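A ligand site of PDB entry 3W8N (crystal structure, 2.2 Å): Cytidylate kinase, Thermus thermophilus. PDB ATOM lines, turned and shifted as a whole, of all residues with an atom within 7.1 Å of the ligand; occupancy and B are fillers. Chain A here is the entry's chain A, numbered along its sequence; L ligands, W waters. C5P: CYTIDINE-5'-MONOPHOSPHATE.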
ATOM      1  N   LYS A  15       9.213  -6.719 -36.929  1.00  0.00           N
ATOM      2  CA  LYS A  15      10.488  -7.371 -36.613  1.00  0.00           C
ATOM      3  C   LYS A  15      10.549  -8.142 -35.296  1.00  0.00           C
ATOM      4  O   LYS A  15      11.219  -9.188 -35.208  1.00  0.00           O
ATOM      5  CB  LYS A  15      11.645  -6.368 -36.680  1.00  0.00           C
ATOM      6  CG  LYS A  15      11.591  -5.262 -35.656  1.00  0.00           C
ATOM      7  CD  LYS A  15      12.808  -4.380 -35.807  1.00  0.00           C
ATOM      8  CE  LYS A  15      12.434  -2.918 -35.896  1.00  0.00           C
ATOM      9  NZ  LYS A  15      11.913  -2.426 -34.617  1.00  0.00           N
ATOM     10  N   SER A  16       9.866  -7.635 -34.281  1.00  0.00           N
ATOM     11  CA  SER A  16       9.863  -8.310 -32.974  1.00  0.00           C
ATOM     12  C   SER A  16       8.980  -9.541 -32.992  1.00  0.00           C
ATOM     13  O   SER A  16       9.369 -10.593 -32.484  1.00  0.00           O
ATOM     14  CB  SER A  16       9.417  -7.347 -31.886  1.00  0.00           C
ATOM     15  OG  SER A  16      10.346  -6.286 -31.794  1.00  0.00           O
ATOM     16  N   ARG A  20      10.444 -13.355 -32.469  1.00  0.00           N
ATOM     17  CA  ARG A  20       9.899 -14.206 -31.421  1.00  0.00           C
ATOM     18  C   ARG A  20       9.443 -15.559 -31.963  1.00  0.00           C
ATOM     19  O   ARG A  20       9.664 -16.572 -31.323  1.00  0.00           O
ATOM     20  CB  ARG A  20       8.759 -13.491 -30.694  1.00  0.00           C
ATOM     21  CG  ARG A  20       8.243 -14.219 -29.451  1.00  0.00           C
ATOM     22  CD  ARG A  20       7.054 -13.477 -28.856  1.00  0.00           C
ATOM     23  NE  ARG A  20       7.360 -12.066 -28.581  1.00  0.00           N
ATOM     24  CZ  ARG A  20       7.963 -11.618 -27.484  1.00  0.00           C
ATOM     25  NH1 ARG A  20       8.334 -12.471 -26.532  1.00  0.00           N
ATOM     26  NH2 ARG A  20       8.194 -10.316 -27.338  1.00  0.00           N
ATOM     27  N   SER A  32      14.787 -10.089 -25.855  1.00  0.00           N
ATOM     28  CA  SER A  32      13.899  -8.930 -25.808  1.00  0.00           C
ATOM     29  C   SER A  32      14.494  -7.931 -24.831  1.00  0.00           C
ATOM     30  O   SER A  32      14.591  -8.205 -23.642  1.00  0.00           O
ATOM     31  CB  SER A  32      12.517  -9.381 -25.313  1.00  0.00           C
ATOM     32  OG  SER A  32      11.581  -8.323 -25.424  1.00  0.00           O
ATOM     33  N   SER A  33      14.895  -6.770 -25.347  1.00  0.00           N
ATOM     34  CA  SER A  33      15.516  -5.694 -24.555  1.00  0.00           C
ATOM     35  C   SER A  33      14.689  -5.203 -23.370  1.00  0.00           C
ATOM     36  O   SER A  33      15.242  -4.776 -22.362  1.00  0.00           O
ATOM     37  CB  SER A  33      15.849  -4.497 -25.450  1.00  0.00           C
ATOM     38  OG  SER A  33      17.124  -4.676 -25.986  1.00  0.00           O
ATOM     39  N   GLY A  34      13.364  -5.228 -23.531  1.00  0.00           N
ATOM     40  CA  GLY A  34      12.470  -4.785 -22.475  1.00  0.00           C
ATOM     41  C   GLY A  34      12.752  -5.260 -21.054  1.00  0.00           C
ATOM     42  O   GLY A  34      12.670  -4.461 -20.112  1.00  0.00           O
ATOM     43  N   LEU A  35      13.108  -6.530 -20.900  1.00  0.00           N
ATOM     44  CA  LEU A  35      13.417  -7.096 -19.587  1.00  0.00           C
ATOM     45  C   LEU A  35      14.574  -6.387 -18.891  1.00  0.00           C
ATOM     46  O   LEU A  35      14.545  -6.191 -17.674  1.00  0.00           O
ATOM     47  CB  LEU A  35      13.738  -8.588 -19.656  1.00  0.00           C
ATOM     48  CG  LEU A  35      12.679  -9.658 -19.432  1.00  0.00           C
ATOM     49  CD1 LEU A  35      13.407 -10.934 -19.037  1.00  0.00           C
ATOM     50  CD2 LEU A  35      11.693  -9.251 -18.346  1.00  0.00           C
ATOM     51  N   LEU A  36      15.600  -6.026 -19.658  1.00  0.00           N
ATOM     52  CA  LEU A  36      16.755  -5.335 -19.093  1.00  0.00           C
ATOM     53  C   LEU A  36      16.412  -3.895 -18.683  1.00  0.00           C
ATOM     54  O   LEU A  36      16.816  -3.435 -17.615  1.00  0.00           O
ATOM     55  CB  LEU A  36      17.950  -5.380 -20.050  1.00  0.00           C
ATOM     56  CG  LEU A  36      18.618  -6.759 -20.111  1.00  0.00           C
ATOM     57  CD1 LEU A  36      19.559  -6.857 -21.294  1.00  0.00           C
ATOM     58  CD2 LEU A  36      19.362  -7.004 -18.802  1.00  0.00           C
ATOM     59  N   TYR A  37      15.649  -3.192 -19.513  1.00  0.00           N
ATOM     60  CA  TYR A  37      15.226  -1.832 -19.168  1.00  0.00           C
ATOM     61  C   TYR A  37      14.363  -1.870 -17.906  1.00  0.00           C
ATOM     62  O   TYR A  37      14.532  -1.042 -17.011  1.00  0.00           O
ATOM     63  CB  TYR A  37      14.485  -1.171 -20.334  1.00  0.00           C
ATOM     64  CG  TYR A  37      15.414  -0.750 -21.460  1.00  0.00           C
ATOM     65  CD1 TYR A  37      16.321   0.308 -21.308  1.00  0.00           C
ATOM     66  CD2 TYR A  37      15.395  -1.431 -22.682  1.00  0.00           C
ATOM     67  CE1 TYR A  37      17.178   0.673 -22.336  1.00  0.00           C
ATOM     68  CE2 TYR A  37      16.268  -1.075 -23.708  1.00  0.00           C
ATOM     69  CZ  TYR A  37      17.146  -0.025 -23.527  1.00  0.00           C
ATOM     70  OH  TYR A  37      17.997   0.296 -24.544  1.00  0.00           O
ATOM     71  N   ARG A  38      13.491  -2.885 -17.804  1.00  0.00           N
ATOM     72  CA  ARG A  38      12.650  -3.068 -16.639  1.00  0.00           C
ATOM     73  C   ARG A  38      13.552  -3.350 -15.419  1.00  0.00           C
ATOM     74  O   ARG A  38      13.354  -2.792 -14.346  1.00  0.00           O
ATOM     75  CB  ARG A  38      11.663  -4.228 -16.846  1.00  0.00           C
ATOM     76  CG  ARG A  38      10.543  -3.903 -17.820  1.00  0.00           C
ATOM     77  CD  ARG A  38       9.697  -5.114 -18.166  1.00  0.00           C
ATOM     78  NE  ARG A  38       8.653  -4.749 -19.137  1.00  0.00           N
ATOM     79  CZ  ARG A  38       7.575  -4.047 -18.827  1.00  0.00           C
ATOM     80  NH1 ARG A  38       7.378  -3.640 -17.592  1.00  0.00           N
ATOM     81  NH2 ARG A  38       6.733  -3.691 -19.782  1.00  0.00           N
ATOM     82  N   LEU A  88       9.503  -7.668 -12.553  1.00  0.00           N
ATOM     83  CA  LEU A  88       9.637  -6.700 -13.630  1.00  0.00           C
ATOM     84  C   LEU A  88       8.433  -6.138 -14.376  1.00  0.00           C
ATOM     85  O   LEU A  88       8.594  -5.247 -15.218  1.00  0.00           O
ATOM     86  CB  LEU A  88      10.653  -7.219 -14.628  1.00  0.00           C
ATOM     87  CG  LEU A  88      11.963  -7.673 -13.960  1.00  0.00           C
ATOM     88  CD1 LEU A  88      12.950  -7.980 -15.026  1.00  0.00           C
ATOM     89  CD2 LEU A  88      12.498  -6.590 -13.032  1.00  0.00           C
ATOM     90  N   HIS A  89       7.232  -6.610 -14.043  1.00  0.00           N
ATOM     91  CA  HIS A  89       6.041  -6.140 -14.724  1.00  0.00           C
ATOM     92  C   HIS A  89       4.984  -5.537 -13.822  1.00  0.00           C
ATOM     93  O   HIS A  89       3.800  -5.558 -14.141  1.00  0.00           O
ATOM     94  CB  HIS A  89       5.458  -7.269 -15.591  1.00  0.00           C
ATOM     95  CG  HIS A  89       6.315  -7.637 -16.759  1.00  0.00           C
ATOM     96  ND1 HIS A  89       7.343  -8.549 -16.657  1.00  0.00           N
ATOM     97  CD2 HIS A  89       6.330  -7.200 -18.037  1.00  0.00           C
ATOM     98  CE1 HIS A  89       7.953  -8.661 -17.824  1.00  0.00           C
ATOM     99  NE2 HIS A  89       7.350  -7.852 -18.684  1.00  0.00           N
ATOM    100  N   ASP A  94       6.440  -0.206 -14.524  1.00  0.00           N
ATOM    101  CA  ASP A  94       5.824   0.298 -15.758  1.00  0.00           C
ATOM    102  C   ASP A  94       5.819   1.822 -15.823  1.00  0.00           C
ATOM    103  O   ASP A  94       6.034   2.406 -16.869  1.00  0.00           O
ATOM    104  CB  ASP A  94       4.361  -0.150 -15.874  1.00  0.00           C
ATOM    105  CG  ASP A  94       4.195  -1.618 -16.312  1.00  0.00           C
ATOM    106  OD1 ASP A  94       5.155  -2.261 -16.756  1.00  0.00           O
ATOM    107  OD2 ASP A  94       3.057  -2.123 -16.222  1.00  0.00           O
ATOM    108  N   VAL A  97       9.707   2.974 -16.388  1.00  0.00           N
ATOM    109  CA  VAL A  97      10.584   2.338 -17.346  1.00  0.00           C
ATOM    110  C   VAL A  97      10.904   3.089 -18.630  1.00  0.00           C
ATOM    111  O   VAL A  97      12.032   3.026 -19.111  1.00  0.00           O
ATOM    112  CB  VAL A  97      10.201   0.871 -17.650  1.00  0.00           C
ATOM    113  CG1 VAL A  97       8.929   0.803 -18.473  1.00  0.00           C
ATOM    114  CG2 VAL A  97      11.366   0.194 -18.401  1.00  0.00           C
ATOM    115  N   SER A  98       9.945   3.822 -19.181  1.00  0.00           N
ATOM    116  CA  SER A  98      10.211   4.559 -20.421  1.00  0.00           C
ATOM    117  C   SER A  98      11.201   5.684 -20.244  1.00  0.00           C
ATOM    118  O   SER A  98      12.110   5.856 -21.062  1.00  0.00           O
ATOM    119  CB  SER A  98       8.922   5.079 -21.048  1.00  0.00           C
ATOM    120  OG  SER A  98       8.147   3.963 -21.477  1.00  0.00           O
ATOM    121  N   ALA A  99      11.077   6.419 -19.140  1.00  0.00           N
ATOM    122  CA  ALA A  99      11.989   7.492 -18.836  1.00  0.00           C
ATOM    123  C   ALA A  99      13.392   6.913 -18.675  1.00  0.00           C
ATOM    124  O   ALA A  99      14.375   7.498 -19.111  1.00  0.00           O
ATOM    125  CB  ALA A  99      11.563   8.209 -17.548  1.00  0.00           C
ATOM    126  N   VAL A 100      13.474   5.751 -18.046  1.00  0.00           N
ATOM    127  CA  VAL A 100      14.773   5.124 -17.860  1.00  0.00           C
ATOM    128  C   VAL A 100      15.414   4.720 -19.204  1.00  0.00           C
ATOM    129  O   VAL A 100      16.605   4.957 -19.425  1.00  0.00           O
ATOM    130  CB  VAL A 100      14.633   3.917 -16.944  1.00  0.00           C
ATOM    131  CG1 VAL A 100      15.872   3.036 -16.993  1.00  0.00           C
ATOM    132  CG2 VAL A 100      14.363   4.396 -15.527  1.00  0.00           C
ATOM    133  N   ALA A 101      14.607   4.159 -20.092  1.00  0.00           N
ATOM    134  CA  ALA A 101      15.055   3.716 -21.415  1.00  0.00           C
ATOM    135  C   ALA A 101      15.464   4.883 -22.313  1.00  0.00           C
ATOM    136  O   ALA A 101      16.117   4.668 -23.328  1.00  0.00           O
ATOM    137  CB  ALA A 101      13.988   2.853 -22.098  1.00  0.00           C
ATOM    138  N   ARG A 102      15.070   6.101 -21.953  1.00  0.00           N
ATOM    139  CA  ARG A 102      15.463   7.269 -22.758  1.00  0.00           C
ATOM    140  C   ARG A 102      16.855   7.770 -22.404  1.00  0.00           C
ATOM    141  O   ARG A 102      17.420   8.586 -23.114  1.00  0.00           O
ATOM    142  CB  ARG A 102      14.443   8.401 -22.644  1.00  0.00           C
ATOM    143  CG  ARG A 102      13.130   8.103 -23.345  1.00  0.00           C
ATOM    144  CD  ARG A 102      12.164   9.271 -23.226  1.00  0.00           C
ATOM    145  NE  ARG A 102      10.781   8.839 -23.082  1.00  0.00           N
ATOM    146  CZ  ARG A 102      10.044   9.019 -21.983  1.00  0.00           C
ATOM    147  NH1 ARG A 102      10.570   9.616 -20.918  1.00  0.00           N
ATOM    148  NH2 ARG A 102       8.798   8.592 -21.947  1.00  0.00           N
ATOM    149  N   ARG A 107      20.921   2.730 -22.205  1.00  0.00           N
ATOM    150  CA  ARG A 107      20.797   1.979 -23.451  1.00  0.00           C
ATOM    151  C   ARG A 107      22.122   1.265 -23.750  1.00  0.00           C
ATOM    152  O   ARG A 107      22.132   0.064 -24.071  1.00  0.00           O
ATOM    153  CB  ARG A 107      20.393   2.895 -24.613  1.00  0.00           C
ATOM    154  CG  ARG A 107      19.029   3.548 -24.402  1.00  0.00           C
ATOM    155  CD  ARG A 107      18.389   4.031 -25.706  1.00  0.00           C
ATOM    156  NE  ARG A 107      17.844   2.940 -26.534  1.00  0.00           N
ATOM    157  CZ  ARG A 107      16.670   2.339 -26.324  1.00  0.00           C
ATOM    158  NH1 ARG A 107      15.890   2.691 -25.311  1.00  0.00           N
ATOM    159  NH2 ARG A 107      16.257   1.385 -27.138  1.00  0.00           N
ATOM    160  N   GLU A 124      17.412  -8.326 -32.308  1.00  0.00           N
ATOM    161  CA  GLU A 124      17.425  -7.240 -33.263  1.00  0.00           C
ATOM    162  C   GLU A 124      18.908  -6.900 -33.394  1.00  0.00           C
ATOM    163  O   GLU A 124      19.629  -6.918 -32.414  1.00  0.00           O
ATOM    164  CB  GLU A 124      16.609  -6.059 -32.751  1.00  0.00           C
ATOM    165  CG  GLU A 124      16.499  -4.929 -33.755  1.00  0.00           C
ATOM    166  CD  GLU A 124      15.571  -3.808 -33.333  1.00  0.00           C
ATOM    167  OE1 GLU A 124      14.720  -4.027 -32.437  1.00  0.00           O
ATOM    168  OE2 GLU A 124      15.669  -2.723 -33.928  1.00  0.00           O
ATOM    169  N   ARG A 126      20.240  -4.083 -34.424  1.00  0.00           N
ATOM    170  CA  ARG A 126      20.501  -2.684 -34.111  1.00  0.00           C
ATOM    171  C   ARG A 126      19.652  -2.126 -32.976  1.00  0.00           C
ATOM    172  O   ARG A 126      18.621  -2.672 -32.625  1.00  0.00           O
ATOM    173  CB  ARG A 126      20.197  -1.844 -35.353  1.00  0.00           C
ATOM    174  CG  ARG A 126      20.931  -2.291 -36.618  1.00  0.00           C
ATOM    175  CD  ARG A 126      20.237  -1.660 -37.815  1.00  0.00           C
ATOM    176  NE  ARG A 126      20.979  -1.824 -39.058  1.00  0.00           N
ATOM    177  CZ  ARG A 126      20.484  -1.518 -40.245  1.00  0.00           C
ATOM    178  NH1 ARG A 126      19.248  -1.031 -40.341  1.00  0.00           N
ATOM    179  NH2 ARG A 126      21.210  -1.679 -41.336  1.00  0.00           N
ATOM    180  N   ASP A 127      20.132  -1.006 -32.424  1.00  0.00           N
ATOM    181  CA  ASP A 127      19.418  -0.239 -31.401  1.00  0.00           C
ATOM    182  C   ASP A 127      19.519   1.163 -31.990  1.00  0.00           C
ATOM    183  O   ASP A 127      20.451   1.913 -31.695  1.00  0.00           O
ATOM    184  CB  ASP A 127      20.124  -0.273 -30.036  1.00  0.00           C
ATOM    185  CG  ASP A 127      19.425   0.626 -28.997  1.00  0.00           C
ATOM    186  OD1 ASP A 127      18.222   0.926 -29.167  1.00  0.00           O
ATOM    187  OD2 ASP A 127      20.077   1.041 -28.028  1.00  0.00           O
HETATM  188  O3P C5P L   1       9.164  -5.700 -21.799  1.00  0.00           O
HETATM  189  P   C5P L   1       8.706  -4.423 -22.656  1.00  0.00           P
HETATM  190  O1P C5P L   1       7.144  -4.143 -22.441  1.00  0.00           O
HETATM  191  O2P C5P L   1       8.966  -4.667 -24.080  1.00  0.00           O
HETATM  192  O5' C5P L   1       9.515  -3.168 -22.118  1.00  0.00           O
HETATM  193  C5' C5P L   1       9.078  -2.100 -22.879  1.00  0.00           C
HETATM  194  C4' C5P L   1       9.753  -0.853 -22.388  1.00  0.00           C
HETATM  195  O4' C5P L   1      11.218  -0.930 -22.429  1.00  0.00           O
HETATM  196  C3' C5P L   1       9.259   0.310 -23.210  1.00  0.00           C
HETATM  197  O3' C5P L   1       8.487   1.189 -22.400  1.00  0.00           O
HETATM  198  C2' C5P L   1      10.519   0.953 -23.776  1.00  0.00           C
HETATM  199  O2' C5P L   1      10.620   2.284 -23.300  1.00  0.00           O
HETATM  200  C1' C5P L   1      11.720   0.084 -23.329  1.00  0.00           C
HETATM  201  N1  C5P L   1      12.343  -0.519 -24.540  1.00  0.00           N
HETATM  202  C2  C5P L   1      13.123   0.223 -25.377  1.00  0.00           C
HETATM  203  N3  C5P L   1      13.681  -0.307 -26.470  1.00  0.00           N
HETATM  204  C4  C5P L   1      13.481  -1.588 -26.775  1.00  0.00           C
HETATM  205  C5  C5P L   1      12.686  -2.382 -25.944  1.00  0.00           C
HETATM  206  C6  C5P L   1      12.130  -1.833 -24.840  1.00  0.00           C
HETATM  207  O2  C5P L   1      13.318   1.402 -25.138  1.00  0.00           O
HETATM  208  N4  C5P L   1      14.050  -2.142 -27.900  1.00  0.00           N
HETATM  209  O   HOH W   1       8.848  -3.429 -26.427  1.00  0.00           O
HETATM  210  O   HOH W   2      11.220  -5.686 -25.562  1.00  0.00           O
HETATM  211  O   HOH W   3      11.041  -8.043 -22.867  1.00  0.00           O
HETATM  212  O   HOH W   4      15.583  -0.536 -30.066  1.00  0.00           O
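The guanidinium group (NH2) of Arg 38 lies within salt-bridge range of an oxygen (O1P) of the ligand.
O2 of the ligand sits at hydrogen-bond distance from NH1 of Arg 107 (2.9 Å).
OG of Ser 98 lies within hydrogen-bond range of O3' of the ligand (2.9 Å).
NE of Arg 38 is in hydrogen-bond range of NE2 of His 89, 3.4 Å away.
OD1 of Asp 94 lies within salt-bridge range of NH1 of Arg 38 (2.7 Å).
The guanidinium group (NH1) of Arg 38 sits at hydrogen-bond distance from the backbone carbonyl oxygen (O) of Leu 88, at 3.1 Å.
The guanidinium group of Arg 107 is in hydrogen-bond range of the backbone carbonyl oxygen of Ala 101, at 2.8 Å.
The guanidinium group (NH1) of Arg 107 lies close to the side-chain hydroxyl (OH) of Tyr 37, 3.3 Å away.
NH2 of Arg 107 lies within salt-bridge range of OD1 of Asp 127.
CB of Ser 33 touches C5 of the ligand (3.8 Å).
Gly 34 touches the ligand (CA to O5', 3.4 Å).
Tyr 37 touches the ligand.
Val 97 touches the ligand.
Ala 101 touches the ligand.
Hydrophobic or aromatic side chains within 4 Å of the ligand: Tyr 37, Val 97 and Ala 101.
Within 4 Å of the ligand: Ser 33, Gly 34, Tyr 37, Arg 38, Val 97, Ser 98, Ala 101 and Arg 107.
Along chain A the residues within 4 Å of the ligand span positions 33 to 107.
The nearest printed residue that does not touch the ligand is Leu 35 (4.1 Å).
Water W2 lies within hydrogen-bond range of the side-chain hydroxyl (OG) of Ser 32 (2.7 Å), an oxygen (O2P) of the ligand (2.9 Å) and the backbone NH (N) of Gly 34 (3.0 Å).
Water W4 bridges N4 of the ligand (3.1 Å) and OD1 of Asp 127 (3.1 Å).
Water W3 lies within hydrogen-bond range of OG of Ser 32, O3P of the ligand and N of Leu 35.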
